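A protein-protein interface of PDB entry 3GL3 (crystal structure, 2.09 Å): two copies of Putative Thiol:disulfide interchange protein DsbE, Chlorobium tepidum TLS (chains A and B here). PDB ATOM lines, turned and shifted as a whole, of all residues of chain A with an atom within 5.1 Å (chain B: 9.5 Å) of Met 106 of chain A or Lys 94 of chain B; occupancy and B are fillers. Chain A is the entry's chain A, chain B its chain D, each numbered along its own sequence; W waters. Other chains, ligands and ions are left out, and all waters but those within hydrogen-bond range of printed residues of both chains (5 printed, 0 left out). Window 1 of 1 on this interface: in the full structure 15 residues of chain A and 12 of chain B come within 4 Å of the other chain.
Of the 13 printed residues of chain A, 7 touch a printed residue of chain B.
Of the 23 printed residues of chain B, 6 touch a printed residue of chain A.
Printed residues of chain B that touch a printed residue of chain A: Leu 69, Ala 71, Pro 93, Lys 94, Pro 98 and Arg 99.
Trp 39 of chain A touches Leu 69 of chain B, but with the chains exchanged Leu 69 of chain A does not touch Trp 39 of chain B (12.6 Å).
Positions printed for both chains: 37, 39 and 69.
Of the 12 pairs that touch across the chains among the printed residues, none has its exchanged pair printed and touching as well.
Of chain B, only Ala 71, Pro 93 and Lys 94 come within 4 Å of Met 106 of chain A.
Lys 94 of chain B touches just these residues of chain A: Val 103 (3.8 Å), Lys 104 (3.96 Å) and Met 106 (3.6 Å).
No residue of chain B comes within 4 Å of Pro 107 of chain A.
Of the printed residues of chain A, Pro 93 of chain B touches Lys 104, Gly 105 and Met 106.
Printed residues of chain A within 4 Å of Pro 98 of chain B: Trp 39.
Of the printed residues of chain B, Gly 105 of chain A touches Ala 71 (3.99 Å) and Pro 93 (3.3 Å).
Printed residues of chain A within 4 Å of Arg 99 of chain B: Leu 69 (3.7 Å).
Printed residues of chain B within 4 Å of Gly 124 of chain A: Ala 71.
Gly 95 of chain B touches none of the printed residues of chain A.
The nearest residue of chain B that does not touch Met 106 of chain A is Gly 95 of chain B (4.6 Å).
The nearest residue of chain A that does not touch Lys 94 of chain B is Gly 105 of chain A (4.5 Å).
Water W4 lies within hydrogen-bond range of the backbone carbonyl oxygen of Pro 93 of chain B, the backbone NH of Met 106 of chain A, the backbone NH of Ala 71 of chain B and the backbone carbonyl oxygen of Leu 69 of chain B.
Water W2 lies within hydrogen-bond range of O of Lys 94 of chain B and SD of Met 106 of chain A.
Water W5 bridges O of Lys 104 of chain A (2.5 Å) and O of Ala 71 of chain B (2.5 Å).
Water W3 lies within hydrogen-bond range of O of Met 106 of chain A, NE1 of Trp 39 of chain B and N of Ala 71 of chain B.
Water W1 lies within hydrogen-bond range of O of Leu 69 of chain A (3.0 Å) and NE of Arg 99 of chain B (3.5 Å).
O of Trp 36 of chain A lies within hydrogen-bond range of N of Leu 69 of chain A (2.7 Å).
OG1 of Thr 108 of chain A is in hydrogen-bond range of O of Gly 105 of chain A, 2.6 Å away.
The side-chain amino group (NZ) of Lys 94 of chain B lies within hydrogen-bond range of the side-chain amide oxygen (OE1) of Gln 96 of chain B (3.3 Å).
The backbone NH of Gly 124 of chain A sits at hydrogen-bond distance from the backbone carbonyl oxygen of Pro 107 of chain A.
The backbone carbonyl oxygen of Met 106 of chain A lies within hydrogen-bond range of the side-chain sulfur of Cys 40 of chain A (3.3 Å).
The backbone carbonyl oxygen (O) of Pro 93 of chain B sits at hydrogen-bond distance from the backbone NH (N) of Met 106 of chain A.
CD1 of Leu 69 of chain B touches CZ3 of Trp 39 of chain A, 3.8 Å away.
CZ2 of Trp 39 of chain A touches CG of Pro 98 of chain B, at 3.8 Å.
Leu 69 of chain A touches Arg 99 of chain B.
O of Lys 104 of chain A touches CB of Pro 93 of chain B (3.3 Å).
Lys 104 of chain A touches Lys 94 of chain B.
Ala 71 of chain B touches Gly 105 of chain A (CB to CA, 3.99 Å).
Gly 105 of chain A touches Pro 93 of chain B (CA to O, 3.3 Å).
Met 106 of chain A touches Ala 71 of chain B (O to CB, 3.4 Å).
Lys 94 of chain B touches Met 106 of chain A (O to CG, 3.6 Å).
CA of Gly 124 of chain A touches CB of Ala 71 of chain B, at 3.9 Å.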
ATOM      1  N   PHE A  35     -33.198  -1.637 -33.266  1.00  0.00           N
ATOM      2  CA  PHE A  35     -32.623  -2.126 -32.025  1.00  0.00           C
ATOM      3  C   PHE A  35     -33.502  -1.531 -30.944  1.00  0.00           C
ATOM      4  O   PHE A  35     -33.526  -0.317 -30.742  1.00  0.00           O
ATOM      5  CB  PHE A  35     -31.162  -1.674 -31.910  1.00  0.00           C
ATOM      6  CG  PHE A  35     -30.239  -2.428 -32.837  1.00  0.00           C
ATOM      7  CD1 PHE A  35     -29.787  -3.700 -32.504  1.00  0.00           C
ATOM      8  CD2 PHE A  35     -29.884  -1.902 -34.064  1.00  0.00           C
ATOM      9  CE1 PHE A  35     -28.999  -4.434 -33.386  1.00  0.00           C
ATOM     10  CE2 PHE A  35     -29.091  -2.633 -34.961  1.00  0.00           C
ATOM     11  CZ  PHE A  35     -28.651  -3.892 -34.625  1.00  0.00           C
ATOM     12  N   TRP A  36     -34.245  -2.399 -30.269  1.00  0.00           N
ATOM     13  CA  TRP A  36     -35.189  -1.970 -29.251  1.00  0.00           C
ATOM     14  C   TRP A  36     -35.161  -2.817 -27.980  1.00  0.00           C
ATOM     15  O   TRP A  36     -34.515  -3.869 -27.926  1.00  0.00           O
ATOM     16  CB  TRP A  36     -36.590  -2.051 -29.829  1.00  0.00           C
ATOM     17  CG  TRP A  36     -37.008  -3.490 -30.060  1.00  0.00           C
ATOM     18  CD1 TRP A  36     -36.595  -4.319 -31.064  1.00  0.00           C
ATOM     19  CD2 TRP A  36     -37.916  -4.253 -29.257  1.00  0.00           C
ATOM     20  NE1 TRP A  36     -37.197  -5.555 -30.940  1.00  0.00           N
ATOM     21  CE2 TRP A  36     -38.013  -5.537 -29.838  1.00  0.00           C
ATOM     22  CE3 TRP A  36     -38.661  -3.972 -28.103  1.00  0.00           C
ATOM     23  CZ2 TRP A  36     -38.832  -6.542 -29.306  1.00  0.00           C
ATOM     24  CZ3 TRP A  36     -39.476  -4.971 -27.571  1.00  0.00           C
ATOM     25  CH2 TRP A  36     -39.555  -6.240 -28.174  1.00  0.00           C
ATOM     26  N   ALA A  37     -35.895  -2.342 -26.972  1.00  0.00           N
ATOM     27  CA  ALA A  37     -36.033  -3.020 -25.684  1.00  0.00           C
ATOM     28  C   ALA A  37     -37.373  -2.615 -25.074  1.00  0.00           C
ATOM     29  O   ALA A  37     -37.853  -1.493 -25.301  1.00  0.00           O
ATOM     30  CB  ALA A  37     -34.882  -2.640 -24.748  1.00  0.00           C
ATOM     31  N   TRP A  39     -38.201  -1.764 -22.106  1.00  0.00           N
ATOM     32  CA  TRP A  39     -38.171  -0.659 -21.148  1.00  0.00           C
ATOM     33  C   TRP A  39     -38.048   0.709 -21.806  1.00  0.00           C
ATOM     34  O   TRP A  39     -38.284   1.735 -21.159  1.00  0.00           O
ATOM     35  CB  TRP A  39     -37.005  -0.824 -20.162  1.00  0.00           C
ATOM     36  CG  TRP A  39     -35.646  -0.967 -20.824  1.00  0.00           C
ATOM     37  CD1 TRP A  39     -34.973  -2.131 -21.069  1.00  0.00           C
ATOM     38  CD2 TRP A  39     -34.834   0.083 -21.359  1.00  0.00           C
ATOM     39  NE1 TRP A  39     -33.792  -1.869 -21.726  1.00  0.00           N
ATOM     40  CE2 TRP A  39     -33.685  -0.519 -21.918  1.00  0.00           C
ATOM     41  CE3 TRP A  39     -34.967   1.476 -21.424  1.00  0.00           C
ATOM     42  CZ2 TRP A  39     -32.675   0.222 -22.531  1.00  0.00           C
ATOM     43  CZ3 TRP A  39     -33.965   2.211 -22.031  1.00  0.00           C
ATOM     44  CH2 TRP A  39     -32.833   1.582 -22.581  1.00  0.00           C
ATOM     45  N   CYS A  40     -37.672   0.724 -23.084  1.00  0.00           N
ATOM     46  CA  CYS A  40     -37.472   1.972 -23.813  1.00  0.00           C
ATOM     47  C   CYS A  40     -38.797   2.560 -24.306  1.00  0.00           C
ATOM     48  O   CYS A  40     -39.405   2.038 -25.233  1.00  0.00           O
ATOM     49  CB  CYS A  40     -36.512   1.727 -24.989  1.00  0.00           C
ATOM     50  SG  CYS A  40     -35.937   3.202 -25.867  1.00  0.00           S
ATOM     51  N   LEU A  69     -33.237  -6.220 -27.338  1.00  0.00           N
ATOM     52  CA  LEU A  69     -32.083  -6.190 -26.454  1.00  0.00           C
ATOM     53  C   LEU A  69     -32.414  -6.319 -24.961  1.00  0.00           C
ATOM     54  O   LEU A  69     -31.600  -5.946 -24.116  1.00  0.00           O
ATOM     55  CB  LEU A  69     -31.287  -4.904 -26.699  1.00  0.00           C
ATOM     56  CG  LEU A  69     -30.798  -4.678 -28.143  1.00  0.00           C
ATOM     57  CD1 LEU A  69     -30.061  -3.347 -28.231  1.00  0.00           C
ATOM     58  CD2 LEU A  69     -29.886  -5.822 -28.570  1.00  0.00           C
ATOM     59  N   VAL A 103     -24.130   0.916 -32.480  1.00  0.00           N
ATOM     60  CA  VAL A 103     -25.324   1.555 -31.927  1.00  0.00           C
ATOM     61  C   VAL A 103     -24.908   2.438 -30.748  1.00  0.00           C
ATOM     62  O   VAL A 103     -24.197   1.980 -29.858  1.00  0.00           O
ATOM     63  CB  VAL A 103     -26.327   0.487 -31.440  1.00  0.00           C
ATOM     64  CG1 VAL A 103     -27.393   1.121 -30.575  1.00  0.00           C
ATOM     65  CG2 VAL A 103     -26.962  -0.219 -32.642  1.00  0.00           C
ATOM     66  N   LYS A 104     -25.355   3.697 -30.738  1.00  0.00           N
ATOM     67  CA  LYS A 104     -25.004   4.635 -29.673  1.00  0.00           C
ATOM     68  C   LYS A 104     -26.209   5.226 -28.953  1.00  0.00           C
ATOM     69  O   LYS A 104     -26.086   6.185 -28.193  1.00  0.00           O
ATOM     70  CB  LYS A 104     -24.156   5.780 -30.238  1.00  0.00           C
ATOM     71  CG  LYS A 104     -22.859   5.306 -30.886  1.00  0.00           C
ATOM     72  CD  LYS A 104     -22.011   6.471 -31.367  1.00  0.00           C
ATOM     73  CE  LYS A 104     -20.827   5.967 -32.185  1.00  0.00           C
ATOM     74  NZ  LYS A 104     -21.288   5.182 -33.382  1.00  0.00           N
ATOM     75  N   GLY A 105     -27.377   4.662 -29.199  1.00  0.00           N
ATOM     76  CA  GLY A 105     -28.572   5.168 -28.553  1.00  0.00           C
ATOM     77  C   GLY A 105     -29.696   4.163 -28.662  1.00  0.00           C
ATOM     78  O   GLY A 105     -29.688   3.297 -29.536  1.00  0.00           O
ATOM     79  N   MET A 106     -30.657   4.262 -27.757  1.00  0.00           N
ATOM     80  CA  MET A 106     -31.785   3.359 -27.771  1.00  0.00           C
ATOM     81  C   MET A 106     -33.074   4.146 -27.892  1.00  0.00           C
ATOM     82  O   MET A 106     -33.376   4.984 -27.065  1.00  0.00           O
ATOM     83  CB  MET A 106     -31.793   2.517 -26.497  1.00  0.00           C
ATOM     84  CG  MET A 106     -30.708   1.458 -26.502  1.00  0.00           C
ATOM     85  SD  MET A 106     -30.983   0.260 -27.821  1.00  0.00           S
ATOM     86  CE  MET A 106     -32.468  -0.524 -27.156  1.00  0.00           C
ATOM     87  N   PRO A 107     -33.851   3.884 -28.944  1.00  0.00           N
ATOM     88  CA  PRO A 107     -33.528   2.893 -29.966  1.00  0.00           C
ATOM     89  C   PRO A 107     -32.625   3.465 -31.054  1.00  0.00           C
ATOM     90  O   PRO A 107     -32.315   4.654 -31.059  1.00  0.00           O
ATOM     91  CB  PRO A 107     -34.895   2.536 -30.519  1.00  0.00           C
ATOM     92  CG  PRO A 107     -35.569   3.870 -30.532  1.00  0.00           C
ATOM     93  CD  PRO A 107     -35.196   4.443 -29.166  1.00  0.00           C
ATOM     94  N   THR A 108     -32.178   2.593 -31.947  1.00  0.00           N
ATOM     95  CA  THR A 108     -31.389   2.997 -33.108  1.00  0.00           C
ATOM     96  C   THR A 108     -31.854   2.060 -34.205  1.00  0.00           C
ATOM     97  O   THR A 108     -32.082   0.866 -33.981  1.00  0.00           O
ATOM     98  CB  THR A 108     -29.859   2.845 -32.927  1.00  0.00           C
ATOM     99  OG1 THR A 108     -29.363   3.876 -32.067  1.00  0.00           O
ATOM    100  CG2 THR A 108     -29.153   2.992 -34.274  1.00  0.00           C
ATOM    101  N   GLY A 124     -32.795   7.230 -31.869  1.00  0.00           N
ATOM    102  CA  GLY A 124     -34.013   7.635 -31.186  1.00  0.00           C
ATOM    103  C   GLY A 124     -35.256   7.536 -32.046  1.00  0.00           C
ATOM    104  O   GLY A 124     -35.192   7.121 -33.195  1.00  0.00           O
ATOM    105  N   ALA B  13     -19.148   1.937 -15.248  1.00  0.00           N
ATOM    106  CA  ALA B  13     -18.323   3.116 -15.474  1.00  0.00           C
ATOM    107  C   ALA B  13     -18.981   3.899 -16.599  1.00  0.00           C
ATOM    108  O   ALA B  13     -18.804   3.580 -17.774  1.00  0.00           O
ATOM    109  CB  ALA B  13     -16.912   2.711 -15.870  1.00  0.00           C
ATOM    110  N   LEU B  14     -19.743   4.921 -16.236  1.00  0.00           N
ATOM    111  CA  LEU B  14     -20.437   5.728 -17.222  1.00  0.00           C
ATOM    112  C   LEU B  14     -19.914   7.147 -17.275  1.00  0.00           C
ATOM    113  O   LEU B  14     -19.396   7.670 -16.280  1.00  0.00           O
ATOM    114  CB  LEU B  14     -21.933   5.760 -16.909  1.00  0.00           C
ATOM    115  CG  LEU B  14     -22.656   4.421 -17.018  1.00  0.00           C
ATOM    116  CD1 LEU B  14     -24.097   4.572 -16.555  1.00  0.00           C
ATOM    117  CD2 LEU B  14     -22.600   3.940 -18.454  1.00  0.00           C
ATOM    118  N   PRO B  15     -20.037   7.796 -18.447  1.00  0.00           N
ATOM    119  CA  PRO B  15     -19.555   9.170 -18.544  1.00  0.00           C
ATOM    120  C   PRO B  15     -20.466  10.053 -17.714  1.00  0.00           C
ATOM    121  O   PRO B  15     -21.679   9.861 -17.665  1.00  0.00           O
ATOM    122  CB  PRO B  15     -19.655   9.475 -20.038  1.00  0.00           C
ATOM    123  CG  PRO B  15     -20.806   8.603 -20.475  1.00  0.00           C
ATOM    124  CD  PRO B  15     -20.508   7.313 -19.756  1.00  0.00           C
ATOM    125  N   ALA B  37     -35.101   9.403 -18.067  1.00  0.00           N
ATOM    126  CA  ALA B  37     -34.904   9.884 -19.427  1.00  0.00           C
ATOM    127  C   ALA B  37     -35.812  11.087 -19.691  1.00  0.00           C
ATOM    128  O   ALA B  37     -36.857  11.231 -19.051  1.00  0.00           O
ATOM    129  CB  ALA B  37     -35.197   8.762 -20.424  1.00  0.00           C
ATOM    130  N   TRP B  39     -37.733  11.645 -22.144  1.00  0.00           N
ATOM    131  CA  TRP B  39     -39.039  11.235 -22.658  1.00  0.00           C
ATOM    132  C   TRP B  39     -39.928  10.612 -21.594  1.00  0.00           C
ATOM    133  O   TRP B  39     -41.061  10.227 -21.880  1.00  0.00           O
ATOM    134  CB  TRP B  39     -38.905  10.248 -23.833  1.00  0.00           C
ATOM    135  CG  TRP B  39     -37.803   9.219 -23.722  1.00  0.00           C
ATOM    136  CD1 TRP B  39     -36.604   9.247 -24.364  1.00  0.00           C
ATOM    137  CD2 TRP B  39     -37.823   7.998 -22.963  1.00  0.00           C
ATOM    138  NE1 TRP B  39     -35.874   8.121 -24.063  1.00  0.00           N
ATOM    139  CE2 TRP B  39     -36.597   7.336 -23.207  1.00  0.00           C
ATOM    140  CE3 TRP B  39     -38.756   7.398 -22.105  1.00  0.00           C
ATOM    141  CZ2 TRP B  39     -36.277   6.104 -22.621  1.00  0.00           C
ATOM    142  CZ3 TRP B  39     -38.436   6.173 -21.520  1.00  0.00           C
ATOM    143  CH2 TRP B  39     -37.206   5.539 -21.785  1.00  0.00           C
ATOM    144  N   VAL B  67     -28.956   7.738 -13.457  1.00  0.00           N
ATOM    145  CA  VAL B  67     -28.477   7.285 -14.757  1.00  0.00           C
ATOM    146  C   VAL B  67     -29.471   7.614 -15.870  1.00  0.00           C
ATOM    147  O   VAL B  67     -30.548   7.022 -15.946  1.00  0.00           O
ATOM    148  CB  VAL B  67     -28.230   5.766 -14.757  1.00  0.00           C
ATOM    149  CG1 VAL B  67     -27.930   5.278 -16.167  1.00  0.00           C
ATOM    150  CG2 VAL B  67     -27.069   5.433 -13.840  1.00  0.00           C
ATOM    151  N   ASN B  68     -29.099   8.558 -16.731  1.00  0.00           N
ATOM    152  CA  ASN B  68     -29.947   8.964 -17.851  1.00  0.00           C
ATOM    153  C   ASN B  68     -29.884   7.973 -19.011  1.00  0.00           C
ATOM    154  O   ASN B  68     -28.815   7.463 -19.354  1.00  0.00           O
ATOM    155  CB  ASN B  68     -29.542  10.345 -18.354  1.00  0.00           C
ATOM    156  CG  ASN B  68     -30.275  10.731 -19.617  1.00  0.00           C
ATOM    157  OD1 ASN B  68     -29.796  10.499 -20.725  1.00  0.00           O
ATOM    158  ND2 ASN B  68     -31.459  11.304 -19.456  1.00  0.00           N
ATOM    159  N   LEU B  69     -31.036   7.721 -19.624  1.00  0.00           N
ATOM    160  CA  LEU B  69     -31.112   6.774 -20.724  1.00  0.00           C
ATOM    161  C   LEU B  69     -31.598   7.344 -22.053  1.00  0.00           C
ATOM    162  O   LEU B  69     -32.083   6.599 -22.898  1.00  0.00           O
ATOM    163  CB  LEU B  69     -31.996   5.594 -20.323  1.00  0.00           C
ATOM    164  CG  LEU B  69     -31.544   4.810 -19.087  1.00  0.00           C
ATOM    165  CD1 LEU B  69     -32.536   3.676 -18.829  1.00  0.00           C
ATOM    166  CD2 LEU B  69     -30.132   4.242 -19.297  1.00  0.00           C
ATOM    167  N   ASP B  70     -31.464   8.654 -22.242  1.00  0.00           N
ATOM    168  CA  ASP B  70     -31.877   9.292 -23.496  1.00  0.00           C
ATOM    169  C   ASP B  70     -30.954   8.895 -24.644  1.00  0.00           C
ATOM    170  O   ASP B  70     -29.733   8.856 -24.476  1.00  0.00           O
ATOM    171  CB  ASP B  70     -31.838  10.815 -23.360  1.00  0.00           C
ATOM    172  CG  ASP B  70     -33.105  11.382 -22.758  1.00  0.00           C
ATOM    173  OD1 ASP B  70     -34.136  11.392 -23.459  1.00  0.00           O
ATOM    174  OD2 ASP B  70     -33.069  11.815 -21.588  1.00  0.00           O
ATOM    175  N   ALA B  71     -31.531   8.604 -25.810  1.00  0.00           N
ATOM    176  CA  ALA B  71     -30.718   8.236 -26.967  1.00  0.00           C
ATOM    177  C   ALA B  71     -29.944   9.469 -27.425  1.00  0.00           C
ATOM    178  O   ALA B  71     -28.846   9.368 -27.965  1.00  0.00           O
ATOM    179  CB  ALA B  71     -31.602   7.716 -28.093  1.00  0.00           C
ATOM    180  N   LYS B  72     -30.524  10.639 -27.200  1.00  0.00           N
ATOM    181  CA  LYS B  72     -29.888  11.895 -27.581  1.00  0.00           C
ATOM    182  C   LYS B  72     -29.580  12.703 -26.324  1.00  0.00           C
ATOM    183  O   LYS B  72     -30.495  13.184 -25.654  1.00  0.00           O
ATOM    184  CB  LYS B  72     -30.814  12.705 -28.491  1.00  0.00           C
ATOM    185  CG  LYS B  72     -30.946  12.182 -29.915  1.00  0.00           C
ATOM    186  CD  LYS B  72     -31.909  13.065 -30.717  1.00  0.00           C
ATOM    187  CE  LYS B  72     -31.897  12.742 -32.205  1.00  0.00           C
ATOM    188  NZ  LYS B  72     -30.580  13.031 -32.830  1.00  0.00           N
ATOM    189  N   THR B  73     -28.299  12.846 -26.000  1.00  0.00           N
ATOM    190  CA  THR B  73     -27.912  13.596 -24.813  1.00  0.00           C
ATOM    191  C   THR B  73     -28.450  15.016 -24.880  1.00  0.00           C
ATOM    192  O   THR B  73     -28.846  15.591 -23.860  1.00  0.00           O
ATOM    193  CB  THR B  73     -26.379  13.622 -24.629  1.00  0.00           C
ATOM    194  OG1 THR B  73     -25.748  13.980 -25.865  1.00  0.00           O
ATOM    195  CG2 THR B  73     -25.875  12.242 -24.174  1.00  0.00           C
ATOM    196  N   ASP B  75     -31.119  15.942 -25.625  1.00  0.00           N
ATOM    197  CA  ASP B  75     -32.419  15.861 -24.966  1.00  0.00           C
ATOM    198  C   ASP B  75     -32.254  15.847 -23.449  1.00  0.00           C
ATOM    199  O   ASP B  75     -33.024  16.474 -22.733  1.00  0.00           O
ATOM    200  CB  ASP B  75     -33.164  14.598 -25.408  1.00  0.00           C
ATOM    201  CG  ASP B  75     -33.648  14.671 -26.851  1.00  0.00           C
ATOM    202  OD1 ASP B  75     -33.974  13.602 -27.417  1.00  0.00           O
ATOM    203  OD2 ASP B  75     -33.714  15.789 -27.413  1.00  0.00           O
ATOM    204  N   PHE B  91     -24.614   9.237 -17.843  1.00  0.00           N
ATOM    205  CA  PHE B  91     -25.307   9.058 -19.116  1.00  0.00           C
ATOM    206  C   PHE B  91     -24.968   7.697 -19.688  1.00  0.00           C
ATOM    207  O   PHE B  91     -23.805   7.311 -19.726  1.00  0.00           O
ATOM    208  CB  PHE B  91     -24.888  10.167 -20.089  1.00  0.00           C
ATOM    209  CG  PHE B  91     -25.168  11.555 -19.579  1.00  0.00           C
ATOM    210  CD1 PHE B  91     -26.390  12.169 -19.828  1.00  0.00           C
ATOM    211  CD2 PHE B  91     -24.227  12.228 -18.805  1.00  0.00           C
ATOM    212  CE1 PHE B  91     -26.680  13.435 -19.307  1.00  0.00           C
ATOM    213  CE2 PHE B  91     -24.503  13.493 -18.279  1.00  0.00           C
ATOM    214  CZ  PHE B  91     -25.732  14.097 -18.531  1.00  0.00           C
ATOM    215  N   ASP B  92     -25.986   6.967 -20.117  1.00  0.00           N
ATOM    216  CA  ASP B  92     -25.789   5.641 -20.679  1.00  0.00           C
ATOM    217  C   ASP B  92     -26.669   5.495 -21.914  1.00  0.00           C
ATOM    218  O   ASP B  92     -27.548   4.637 -21.955  1.00  0.00           O
ATOM    219  CB  ASP B  92     -26.155   4.582 -19.632  1.00  0.00           C
ATOM    220  CG  ASP B  92     -25.822   3.163 -20.075  1.00  0.00           C
ATOM    221  OD1 ASP B  92     -25.273   2.978 -21.181  1.00  0.00           O
ATOM    222  OD2 ASP B  92     -26.111   2.228 -19.301  1.00  0.00           O
ATOM    223  N   PRO B  93     -26.445   6.336 -22.941  1.00  0.00           N
ATOM    224  CA  PRO B  93     -27.256   6.261 -24.166  1.00  0.00           C
ATOM    225  C   PRO B  93     -27.352   4.866 -24.779  1.00  0.00           C
ATOM    226  O   PRO B  93     -28.387   4.490 -25.325  1.00  0.00           O
ATOM    227  CB  PRO B  93     -26.578   7.270 -25.100  1.00  0.00           C
ATOM    228  CG  PRO B  93     -25.184   7.368 -24.572  1.00  0.00           C
ATOM    229  CD  PRO B  93     -25.400   7.363 -23.081  1.00  0.00           C
ATOM    230  N   LYS B  94     -26.276   4.099 -24.693  1.00  0.00           N
ATOM    231  CA  LYS B  94     -26.287   2.756 -25.240  1.00  0.00           C
ATOM    232  C   LYS B  94     -27.197   1.837 -24.428  1.00  0.00           C
ATOM    233  O   LYS B  94     -27.573   0.762 -24.889  1.00  0.00           O
ATOM    234  CB  LYS B  94     -24.866   2.201 -25.295  1.00  0.00           C
ATOM    235  CG  LYS B  94     -23.958   3.013 -26.212  1.00  0.00           C
ATOM    236  CD  LYS B  94     -22.626   2.333 -26.460  1.00  0.00           C
ATOM    237  CE  LYS B  94     -21.866   2.118 -25.168  1.00  0.00           C
ATOM    238  NZ  LYS B  94     -21.590   3.406 -24.461  1.00  0.00           N
ATOM    239  N   GLY B  95     -27.558   2.270 -23.221  1.00  0.00           N
ATOM    240  CA  GLY B  95     -28.435   1.474 -22.380  1.00  0.00           C
ATOM    241  C   GLY B  95     -27.824   0.204 -21.819  1.00  0.00           C
ATOM    242  O   GLY B  95     -28.506  -0.804 -21.665  1.00  0.00           O
ATOM    243  N   GLN B  96     -26.538   0.262 -21.496  1.00  0.00           N
ATOM    244  CA  GLN B  96     -25.806  -0.870 -20.940  1.00  0.00           C
ATOM    245  C   GLN B  96     -26.229  -1.238 -19.513  1.00  0.00           C
ATOM    246  O   GLN B  96     -26.451  -2.412 -19.205  1.00  0.00           O
ATOM    247  CB  GLN B  96     -24.312  -0.556 -20.949  1.00  0.00           C
ATOM    248  CG  GLN B  96     -23.764  -0.249 -22.333  1.00  0.00           C
ATOM    249  CD  GLN B  96     -22.439   0.487 -22.291  1.00  0.00           C
ATOM    250  OE1 GLN B  96     -22.357   1.617 -21.795  1.00  0.00           O
ATOM    251  NE2 GLN B  96     -21.392  -0.148 -22.809  1.00  0.00           N
ATOM    252  N   THR B  97     -26.335  -0.239 -18.643  1.00  0.00           N
ATOM    253  CA  THR B  97     -26.702  -0.490 -17.255  1.00  0.00           C
ATOM    254  C   THR B  97     -28.135  -0.989 -17.061  1.00  0.00           C
ATOM    255  O   THR B  97     -28.383  -1.852 -16.225  1.00  0.00           O
ATOM    256  CB  THR B  97     -26.438   0.756 -16.376  1.00  0.00           C
ATOM    257  OG1 THR B  97     -27.160   1.885 -16.884  1.00  0.00           O
ATOM    258  CG2 THR B  97     -24.954   1.083 -16.371  1.00  0.00           C
ATOM    259  N   PRO B  98     -29.101  -0.452 -17.822  1.00  0.00           N
ATOM    260  CA  PRO B  98     -30.462  -0.955 -17.622  1.00  0.00           C
ATOM    261  C   PRO B  98     -30.568  -2.434 -18.005  1.00  0.00           C
ATOM    262  O   PRO B  98     -31.451  -3.155 -17.528  1.00  0.00           O
ATOM    263  CB  PRO B  98     -31.304  -0.045 -18.517  1.00  0.00           C
ATOM    264  CG  PRO B  98     -30.333   0.395 -19.580  1.00  0.00           C
ATOM    265  CD  PRO B  98     -29.090   0.666 -18.781  1.00  0.00           C
ATOM    266  N   ARG B  99     -29.659  -2.881 -18.865  1.00  0.00           N
ATOM    267  CA  ARG B  99     -29.639  -4.271 -19.295  1.00  0.00           C
ATOM    268  C   ARG B  99     -29.054  -5.129 -18.169  1.00  0.00           C
ATOM    269  O   ARG B  99     -29.523  -6.236 -17.901  1.00  0.00           O
ATOM    270  CB  ARG B  99     -28.796  -4.413 -20.572  1.00  0.00           C
ATOM    271  CG  ARG B  99     -28.696  -5.833 -21.100  1.00  0.00           C
ATOM    272  CD  ARG B  99     -28.197  -5.892 -22.544  1.00  0.00           C
ATOM    273  NE  ARG B  99     -26.788  -5.534 -22.697  1.00  0.00           N
ATOM    274  CZ  ARG B  99     -26.345  -4.493 -23.403  1.00  0.00           C
ATOM    275  NH1 ARG B  99     -27.200  -3.692 -24.031  1.00  0.00           N
ATOM    276  NH2 ARG B  99     -25.043  -4.253 -23.491  1.00  0.00           N
ATOM    277  N   LEU B 100     -28.029  -4.602 -17.504  1.00  0.00           N
ATOM    278  CA  LEU B 100     -27.386  -5.313 -16.407  1.00  0.00           C
ATOM    279  C   LEU B 100     -28.316  -5.392 -15.210  1.00  0.00           C
ATOM    280  O   LEU B 100     -28.288  -6.361 -14.454  1.00  0.00           O
ATOM    281  CB  LEU B 100     -26.093  -4.603 -15.996  1.00  0.00           C
ATOM    282  CG  LEU B 100     -24.983  -4.495 -17.042  1.00  0.00           C
ATOM    283  CD1 LEU B 100     -23.772  -3.805 -16.423  1.00  0.00           C
ATOM    284  CD2 LEU B 100     -24.605  -5.877 -17.544  1.00  0.00           C
HETATM  285  O   HOH W   1     -28.942  -7.252 -24.833  1.00  0.00           O
HETATM  286  O   HOH W   2     -27.788  -0.651 -26.928  1.00  0.00           O
HETATM  287  O   HOH W   3     -34.144   7.435 -26.171  1.00  0.00           O
HETATM  288  O   HOH W   4     -30.562   5.600 -25.520  1.00  0.00           O
HETATM  289  O   HOH W   5     -26.602   8.574 -28.872  1.00  0.00           O
